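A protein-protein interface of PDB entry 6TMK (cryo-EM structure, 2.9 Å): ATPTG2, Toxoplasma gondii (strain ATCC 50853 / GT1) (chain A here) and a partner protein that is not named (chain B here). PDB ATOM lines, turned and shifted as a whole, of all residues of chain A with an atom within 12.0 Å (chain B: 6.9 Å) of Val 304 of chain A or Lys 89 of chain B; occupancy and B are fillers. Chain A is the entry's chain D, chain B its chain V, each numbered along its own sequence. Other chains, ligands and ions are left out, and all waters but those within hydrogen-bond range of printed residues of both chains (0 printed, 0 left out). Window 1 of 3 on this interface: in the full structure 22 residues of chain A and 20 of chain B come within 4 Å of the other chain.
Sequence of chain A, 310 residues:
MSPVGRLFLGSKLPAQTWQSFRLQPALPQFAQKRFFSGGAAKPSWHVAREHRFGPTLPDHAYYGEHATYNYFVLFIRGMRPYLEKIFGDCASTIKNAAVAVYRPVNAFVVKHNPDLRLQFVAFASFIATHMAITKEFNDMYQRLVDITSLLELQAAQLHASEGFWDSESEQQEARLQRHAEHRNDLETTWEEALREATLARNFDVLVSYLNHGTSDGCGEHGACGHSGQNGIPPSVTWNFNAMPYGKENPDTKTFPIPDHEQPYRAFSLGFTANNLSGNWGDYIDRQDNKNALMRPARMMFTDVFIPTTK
The side-chain amide oxygen of Gln 88 of chain B lies close to the side-chain carboxylate of Asp 303 of chain A (3.5 Å).
Among the printed residues, merely in contact across the chains: Val 304 of chain A with Val 85 of chain B (3.4 Å), Ile 306 of chain A with Gln 93 of chain B (3.8 Å), Asp 303 of chain A with Val 85 of chain B (3.9 Å), Val 304 of chain A with Lys 89 of chain B (3.9 Å) and Ile 306 of chain A with Lys 89 of chain B (3.998 Å).
Of chain B, only Val 85 and Lys 89 come within 4 Å of Val 304 of chain A. Of the printed residues of chain A, Lys 89 of chain B touches Val 304 (3.9 Å) and Ile 306 (3.998 Å). Gln 88 of chain B touches one residue of chain A. Printed residues of chain B within 4 Å of Asp 303 of chain A: Val 85 (3.9 Å) and Gln 88 (3.4 Å). Printed residues of chain B within 4 Å of Ile 306 of chain A: Lys 89 and Gln 93. Met 299 of chain A touches none of the printed residues of chain B. The nearest printed residue of chain A that does not touch Lys 89 of chain B is Phe 305 of chain A (5.7 Å).
Of the 14 printed residues of chain A, 3 touch a printed residue of chain B. Printed residues of chain A that touch a printed residue of chain B: Asp 303, Val 304 and Ile 306. Among the printed residues, no Asp or Glu carboxylate lies within 4 Å of a Lys or Arg side-chain nitrogen of the other chain.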
ATOM      1  N   ASN A 289      11.122 -20.269  20.213  1.00  0.00           N
ATOM      2  CA  ASN A 289      10.395 -21.275  19.449  1.00  0.00           C
ATOM      3  C   ASN A 289      11.331 -22.343  18.900  1.00  0.00           C
ATOM      4  O   ASN A 289      10.979 -23.528  18.870  1.00  0.00           O
ATOM      5  CB  ASN A 289       9.601 -20.616  18.326  1.00  0.00           C
ATOM      6  CG  ASN A 289      10.437 -19.670  17.498  1.00  0.00           C
ATOM      7  OD1 ASN A 289      11.235 -18.900  18.027  1.00  0.00           O
ATOM      8  ND2 ASN A 289      10.260 -19.725  16.190  1.00  0.00           N
ATOM      9  N   LYS A 290      12.517 -21.946  18.452  1.00  0.00           N
ATOM     10  CA  LYS A 290      13.472 -22.887  17.893  1.00  0.00           C
ATOM     11  C   LYS A 290      14.250 -23.581  18.999  1.00  0.00           C
ATOM     12  O   LYS A 290      14.413 -23.053  20.102  1.00  0.00           O
ATOM     13  CB  LYS A 290      14.445 -22.180  16.953  1.00  0.00           C
ATOM     14  CG  LYS A 290      13.788 -21.457  15.809  1.00  0.00           C
ATOM     15  CD  LYS A 290      13.121 -22.414  14.866  1.00  0.00           C
ATOM     16  CE  LYS A 290      12.439 -21.684  13.747  1.00  0.00           C
ATOM     17  NZ  LYS A 290      11.434 -22.554  13.095  1.00  0.00           N
ATOM     18  N   ALA A 297      21.480 -20.922  13.823  1.00  0.00           N
ATOM     19  CA  ALA A 297      21.164 -20.734  12.412  1.00  0.00           C
ATOM     20  C   ALA A 297      19.744 -20.214  12.204  1.00  0.00           C
ATOM     21  O   ALA A 297      19.052 -20.611  11.268  1.00  0.00           O
ATOM     22  CB  ALA A 297      21.359 -22.032  11.646  1.00  0.00           C
ATOM     23  N   ARG A 298      19.303 -19.299  13.068  1.00  0.00           N
ATOM     24  CA  ARG A 298      17.952 -18.759  12.970  1.00  0.00           C
ATOM     25  C   ARG A 298      17.744 -17.979  11.681  1.00  0.00           C
ATOM     26  O   ARG A 298      16.631 -17.940  11.150  1.00  0.00           O
ATOM     27  CB  ARG A 298      17.691 -17.863  14.174  1.00  0.00           C
ATOM     28  CG  ARG A 298      16.261 -17.464  14.413  1.00  0.00           C
ATOM     29  CD  ARG A 298      16.228 -16.319  15.381  1.00  0.00           C
ATOM     30  NE  ARG A 298      16.934 -16.668  16.604  1.00  0.00           N
ATOM     31  CZ  ARG A 298      16.452 -17.484  17.533  1.00  0.00           C
ATOM     32  NH1 ARG A 298      15.254 -18.024  17.391  1.00  0.00           N
ATOM     33  NH2 ARG A 298      17.173 -17.759  18.607  1.00  0.00           N
ATOM     34  N   MET A 299      18.802 -17.357  11.171  1.00  0.00           N
ATOM     35  CA  MET A 299      18.713 -16.579   9.943  1.00  0.00           C
ATOM     36  C   MET A 299      18.231 -17.416   8.767  1.00  0.00           C
ATOM     37  O   MET A 299      17.641 -16.881   7.823  1.00  0.00           O
ATOM     38  CB  MET A 299      20.073 -15.978   9.636  1.00  0.00           C
ATOM     39  CG  MET A 299      20.065 -14.882   8.622  1.00  0.00           C
ATOM     40  SD  MET A 299      21.734 -14.547   8.060  1.00  0.00           S
ATOM     41  CE  MET A 299      21.481 -12.931   7.371  1.00  0.00           C
ATOM     42  N   MET A 300      18.456 -18.725   8.811  1.00  0.00           N
ATOM     43  CA  MET A 300      18.106 -19.606   7.708  1.00  0.00           C
ATOM     44  C   MET A 300      16.637 -19.988   7.692  1.00  0.00           C
ATOM     45  O   MET A 300      16.165 -20.523   6.687  1.00  0.00           O
ATOM     46  CB  MET A 300      18.959 -20.862   7.794  1.00  0.00           C
ATOM     47  CG  MET A 300      20.400 -20.624   7.429  1.00  0.00           C
ATOM     48  SD  MET A 300      21.469 -21.975   7.933  1.00  0.00           S
ATOM     49  CE  MET A 300      20.742 -23.278   6.975  1.00  0.00           C
ATOM     50  N   PHE A 301      15.917 -19.750   8.782  1.00  0.00           N
ATOM     51  CA  PHE A 301      14.496 -20.031   8.882  1.00  0.00           C
ATOM     52  C   PHE A 301      13.655 -18.765   8.764  1.00  0.00           C
ATOM     53  O   PHE A 301      12.595 -18.665   9.386  1.00  0.00           O
ATOM     54  CB  PHE A 301      14.228 -20.758  10.194  1.00  0.00           C
ATOM     55  CG  PHE A 301      15.122 -21.939  10.402  1.00  0.00           C
ATOM     56  CD1 PHE A 301      14.842 -23.142   9.798  1.00  0.00           C
ATOM     57  CD2 PHE A 301      16.264 -21.835  11.168  1.00  0.00           C
ATOM     58  CE1 PHE A 301      15.667 -24.220   9.970  1.00  0.00           C
ATOM     59  CE2 PHE A 301      17.089 -22.913  11.338  1.00  0.00           C
ATOM     60  CZ  PHE A 301      16.789 -24.106  10.738  1.00  0.00           C
ATOM     61  N   THR A 302      14.100 -17.804   7.955  1.00  0.00           N
ATOM     62  CA  THR A 302      13.453 -16.508   7.847  1.00  0.00           C
ATOM     63  C   THR A 302      13.440 -16.039   6.402  1.00  0.00           C
ATOM     64  O   THR A 302      14.402 -16.255   5.663  1.00  0.00           O
ATOM     65  CB  THR A 302      14.175 -15.451   8.691  1.00  0.00           C
ATOM     66  OG1 THR A 302      15.494 -15.241   8.179  1.00  0.00           O
ATOM     67  CG2 THR A 302      14.279 -15.893  10.117  1.00  0.00           C
ATOM     68  N   ASP A 303      12.340 -15.402   6.004  1.00  0.00           N
ATOM     69  CA  ASP A 303      12.306 -14.726   4.714  1.00  0.00           C
ATOM     70  C   ASP A 303      12.964 -13.351   4.779  1.00  0.00           C
ATOM     71  O   ASP A 303      13.487 -12.874   3.769  1.00  0.00           O
ATOM     72  CB  ASP A 303      10.860 -14.610   4.236  1.00  0.00           C
ATOM     73  CG  ASP A 303      10.439 -15.775   3.365  1.00  0.00           C
ATOM     74  OD1 ASP A 303      11.264 -16.242   2.553  1.00  0.00           O
ATOM     75  OD2 ASP A 303       9.283 -16.227   3.494  1.00  0.00           O
ATOM     76  N   VAL A 304      12.942 -12.704   5.943  1.00  0.00           N
ATOM     77  CA  VAL A 304      13.590 -11.418   6.154  1.00  0.00           C
ATOM     78  C   VAL A 304      14.210 -11.441   7.541  1.00  0.00           C
ATOM     79  O   VAL A 304      13.721 -12.117   8.449  1.00  0.00           O
ATOM     80  CB  VAL A 304      12.624 -10.217   6.010  1.00  0.00           C
ATOM     81  CG1 VAL A 304      12.301  -9.962   4.585  1.00  0.00           C
ATOM     82  CG2 VAL A 304      11.350 -10.473   6.746  1.00  0.00           C
ATOM     83  N   PHE A 305      15.283 -10.673   7.707  1.00  0.00           N
ATOM     84  CA  PHE A 305      16.007 -10.639   8.967  1.00  0.00           C
ATOM     85  C   PHE A 305      16.560  -9.237   9.160  1.00  0.00           C
ATOM     86  O   PHE A 305      17.264  -8.726   8.285  1.00  0.00           O
ATOM     87  CB  PHE A 305      17.135 -11.674   8.981  1.00  0.00           C
ATOM     88  CG  PHE A 305      17.580 -12.075  10.348  1.00  0.00           C
ATOM     89  CD1 PHE A 305      18.661 -11.468  10.945  1.00  0.00           C
ATOM     90  CD2 PHE A 305      16.940 -13.093  11.023  1.00  0.00           C
ATOM     91  CE1 PHE A 305      19.068 -11.843  12.188  1.00  0.00           C
ATOM     92  CE2 PHE A 305      17.354 -13.476  12.271  1.00  0.00           C
ATOM     93  CZ  PHE A 305      18.420 -12.857  12.850  1.00  0.00           C
ATOM     94  N   ILE A 306      16.239  -8.628  10.291  1.00  0.00           N
ATOM     95  CA  ILE A 306      16.695  -7.291  10.645  1.00  0.00           C
ATOM     96  C   ILE A 306      17.547  -7.395  11.905  1.00  0.00           C
ATOM     97  O   ILE A 306      17.023  -7.483  13.015  1.00  0.00           O
ATOM     98  CB  ILE A 306      15.525  -6.315  10.846  1.00  0.00           C
ATOM     99  CG1 ILE A 306      14.829  -6.033   9.526  1.00  0.00           C
ATOM    100  CG2 ILE A 306      16.022  -5.028  11.425  1.00  0.00           C
ATOM    101  CD1 ILE A 306      13.422  -5.664   9.688  1.00  0.00           C
ATOM    102  N   PRO A 307      18.869  -7.400  11.773  1.00  0.00           N
ATOM    103  CA  PRO A 307      19.722  -7.712  12.921  1.00  0.00           C
ATOM    104  C   PRO A 307      19.733  -6.607  13.962  1.00  0.00           C
ATOM    105  O   PRO A 307      19.185  -5.517  13.788  1.00  0.00           O
ATOM    106  CB  PRO A 307      21.109  -7.854  12.292  1.00  0.00           C
ATOM    107  CG  PRO A 307      20.872  -8.067  10.869  1.00  0.00           C
ATOM    108  CD  PRO A 307      19.674  -7.262  10.555  1.00  0.00           C
ATOM    109  N   THR A 308      20.398  -6.919  15.065  1.00  0.00           N
ATOM    110  CA  THR A 308      20.527  -6.012  16.186  1.00  0.00           C
ATOM    111  C   THR A 308      21.410  -4.822  15.837  1.00  0.00           C
ATOM    112  O   THR A 308      22.115  -4.796  14.827  1.00  0.00           O
ATOM    113  CB  THR A 308      21.144  -6.720  17.385  1.00  0.00           C
ATOM    114  OG1 THR A 308      22.461  -7.162  17.042  1.00  0.00           O
ATOM    115  CG2 THR A 308      20.323  -7.893  17.786  1.00  0.00           C
ATOM    116  N   MET B  84       5.623  -9.758  -1.778  1.00  0.00           N
ATOM    117  CA  MET B  84       5.128 -10.452  -0.602  1.00  0.00           C
ATOM    118  C   MET B  84       6.148 -10.424   0.528  1.00  0.00           C
ATOM    119  O   MET B  84       5.785 -10.245   1.691  1.00  0.00           O
ATOM    120  CB  MET B  84       4.761 -11.887  -0.972  1.00  0.00           C
ATOM    121  CG  MET B  84       4.169 -12.709   0.158  1.00  0.00           C
ATOM    122  SD  MET B  84       2.723 -11.970   0.935  1.00  0.00           S
ATOM    123  CE  MET B  84       1.546 -12.080  -0.400  1.00  0.00           C
ATOM    124  N   VAL B  85       7.432 -10.587   0.204  1.00  0.00           N
ATOM    125  CA  VAL B  85       8.462 -10.551   1.235  1.00  0.00           C
ATOM    126  C   VAL B  85       8.630  -9.135   1.775  1.00  0.00           C
ATOM    127  O   VAL B  85       8.933  -8.944   2.957  1.00  0.00           O
ATOM    128  CB  VAL B  85       9.775 -11.128   0.682  1.00  0.00           C
ATOM    129  CG1 VAL B  85      10.900 -10.948   1.662  1.00  0.00           C
ATOM    130  CG2 VAL B  85       9.604 -12.588   0.344  1.00  0.00           C
ATOM    131  N   ARG B  86       8.435  -8.125   0.928  1.00  0.00           N
ATOM    132  CA  ARG B  86       8.416  -6.738   1.386  1.00  0.00           C
ATOM    133  C   ARG B  86       7.284  -6.512   2.386  1.00  0.00           C
ATOM    134  O   ARG B  86       7.479  -5.912   3.456  1.00  0.00           O
ATOM    135  CB  ARG B  86       8.290  -5.826   0.166  1.00  0.00           C
ATOM    136  CG  ARG B  86       8.037  -4.372   0.417  1.00  0.00           C
ATOM    137  CD  ARG B  86       9.169  -3.700   1.117  1.00  0.00           C
ATOM    138  NE  ARG B  86       8.895  -2.282   1.285  1.00  0.00           N
ATOM    139  CZ  ARG B  86       9.679  -1.442   1.942  1.00  0.00           C
ATOM    140  NH1 ARG B  86      10.800  -1.870   2.496  1.00  0.00           N
ATOM    141  NH2 ARG B  86       9.339  -0.172   2.043  1.00  0.00           N
ATOM    142  N   LYS B  87       6.086  -6.987   2.045  1.00  0.00           N
ATOM    143  CA  LYS B  87       4.957  -6.902   2.964  1.00  0.00           C
ATOM    144  C   LYS B  87       5.245  -7.651   4.259  1.00  0.00           C
ATOM    145  O   LYS B  87       4.847  -7.212   5.341  1.00  0.00           O
ATOM    146  CB  LYS B  87       3.707  -7.452   2.288  1.00  0.00           C
ATOM    147  CG  LYS B  87       2.426  -7.273   3.057  1.00  0.00           C
ATOM    148  CD  LYS B  87       1.240  -7.520   2.186  1.00  0.00           C
ATOM    149  CE  LYS B  87       1.210  -8.937   1.708  1.00  0.00           C
ATOM    150  NZ  LYS B  87      -0.170  -9.365   1.445  1.00  0.00           N
ATOM    151  N   GLN B  88       5.914  -8.797   4.159  1.00  0.00           N
ATOM    152  CA  GLN B  88       6.293  -9.563   5.339  1.00  0.00           C
ATOM    153  C   GLN B  88       7.262  -8.792   6.221  1.00  0.00           C
ATOM    154  O   GLN B  88       7.170  -8.846   7.447  1.00  0.00           O
ATOM    155  CB  GLN B  88       6.925 -10.873   4.907  1.00  0.00           C
ATOM    156  CG  GLN B  88       5.963 -11.869   4.403  1.00  0.00           C
ATOM    157  CD  GLN B  88       6.644 -13.046   3.787  1.00  0.00           C
ATOM    158  OE1 GLN B  88       7.861 -13.074   3.650  1.00  0.00           O
ATOM    159  NE2 GLN B  88       5.868 -14.036   3.420  1.00  0.00           N
ATOM    160  N   LYS B  89       8.215  -8.096   5.613  1.00  0.00           N
ATOM    161  CA  LYS B  89       9.132  -7.260   6.373  1.00  0.00           C
ATOM    162  C   LYS B  89       8.375  -6.195   7.149  1.00  0.00           C
ATOM    163  O   LYS B  89       8.609  -5.980   8.349  1.00  0.00           O
ATOM    164  CB  LYS B  89      10.140  -6.622   5.429  1.00  0.00           C
ATOM    165  CG  LYS B  89      11.350  -6.079   6.105  1.00  0.00           C
ATOM    166  CD  LYS B  89      12.151  -5.244   5.159  1.00  0.00           C
ATOM    167  CE  LYS B  89      13.404  -4.733   5.800  1.00  0.00           C
ATOM    168  NZ  LYS B  89      14.580  -4.908   4.932  1.00  0.00           N
ATOM    169  N   LYS B  90       7.467  -5.506   6.465  1.00  0.00           N
ATOM    170  CA  LYS B  90       6.685  -4.477   7.132  1.00  0.00           C
ATOM    171  C   LYS B  90       5.844  -5.061   8.261  1.00  0.00           C
ATOM    172  O   LYS B  90       5.763  -4.478   9.348  1.00  0.00           O
ATOM    173  CB  LYS B  90       5.823  -3.751   6.114  1.00  0.00           C
ATOM    174  CG  LYS B  90       6.628  -3.127   5.017  1.00  0.00           C
ATOM    175  CD  LYS B  90       5.951  -1.945   4.398  1.00  0.00           C
ATOM    176  CE  LYS B  90       5.368  -2.270   3.076  1.00  0.00           C
ATOM    177  NZ  LYS B  90       4.601  -1.121   2.575  1.00  0.00           N
ATOM    178  N   THR B  91       5.208  -6.206   8.022  1.00  0.00           N
ATOM    179  CA  THR B  91       4.395  -6.843   9.050  1.00  0.00           C
ATOM    180  C   THR B  91       5.251  -7.284  10.228  1.00  0.00           C
ATOM    181  O   THR B  91       4.816  -7.214  11.380  1.00  0.00           O
ATOM    182  CB  THR B  91       3.635  -8.025   8.453  1.00  0.00           C
ATOM    183  OG1 THR B  91       3.017  -7.624   7.229  1.00  0.00           O
ATOM    184  CG2 THR B  91       2.588  -8.527   9.404  1.00  0.00           C
ATOM    185  N   ALA B  92       6.475  -7.726   9.958  1.00  0.00           N
ATOM    186  CA  ALA B  92       7.378  -8.131  11.023  1.00  0.00           C
ATOM    187  C   ALA B  92       7.710  -6.948  11.914  1.00  0.00           C
ATOM    188  O   ALA B  92       7.661  -7.050  13.144  1.00  0.00           O
ATOM    189  CB  ALA B  92       8.640  -8.742  10.425  1.00  0.00           C
ATOM    190  N   GLN B  93       8.057  -5.815  11.307  1.00  0.00           N
ATOM    191  CA  GLN B  93       8.380  -4.631  12.096  1.00  0.00           C
ATOM    192  C   GLN B  93       7.162  -4.147  12.873  1.00  0.00           C
ATOM    193  O   GLN B  93       7.276  -3.714  14.026  1.00  0.00           O
ATOM    194  CB  GLN B  93       8.932  -3.537  11.198  1.00  0.00           C
ATOM    195  CG  GLN B  93      10.236  -3.883  10.574  1.00  0.00           C
ATOM    196  CD  GLN B  93      10.898  -2.714   9.910  1.00  0.00           C
ATOM    197  OE1 GLN B  93      11.599  -1.932  10.546  1.00  0.00           O
ATOM    198  NE2 GLN B  93      10.689  -2.589   8.615  1.00  0.00           N
ATOM    199  N   LEU B  94       5.984  -4.230  12.259  1.00  0.00           N
ATOM    200  CA  LEU B  94       4.749  -3.851  12.931  1.00  0.00           C
ATOM    201  C   LEU B  94       4.513  -4.702  14.170  1.00  0.00           C
ATOM    202  O   LEU B  94       4.238  -4.182  15.260  1.00  0.00           O
ATOM    203  CB  LEU B  94       3.598  -4.023  11.952  1.00  0.00           C
ATOM    204  CG  LEU B  94       2.171  -3.681  12.353  1.00  0.00           C
ATOM    205  CD1 LEU B  94       2.017  -2.215  12.591  1.00  0.00           C
ATOM    206  CD2 LEU B  94       1.242  -4.172  11.302  1.00  0.00           C
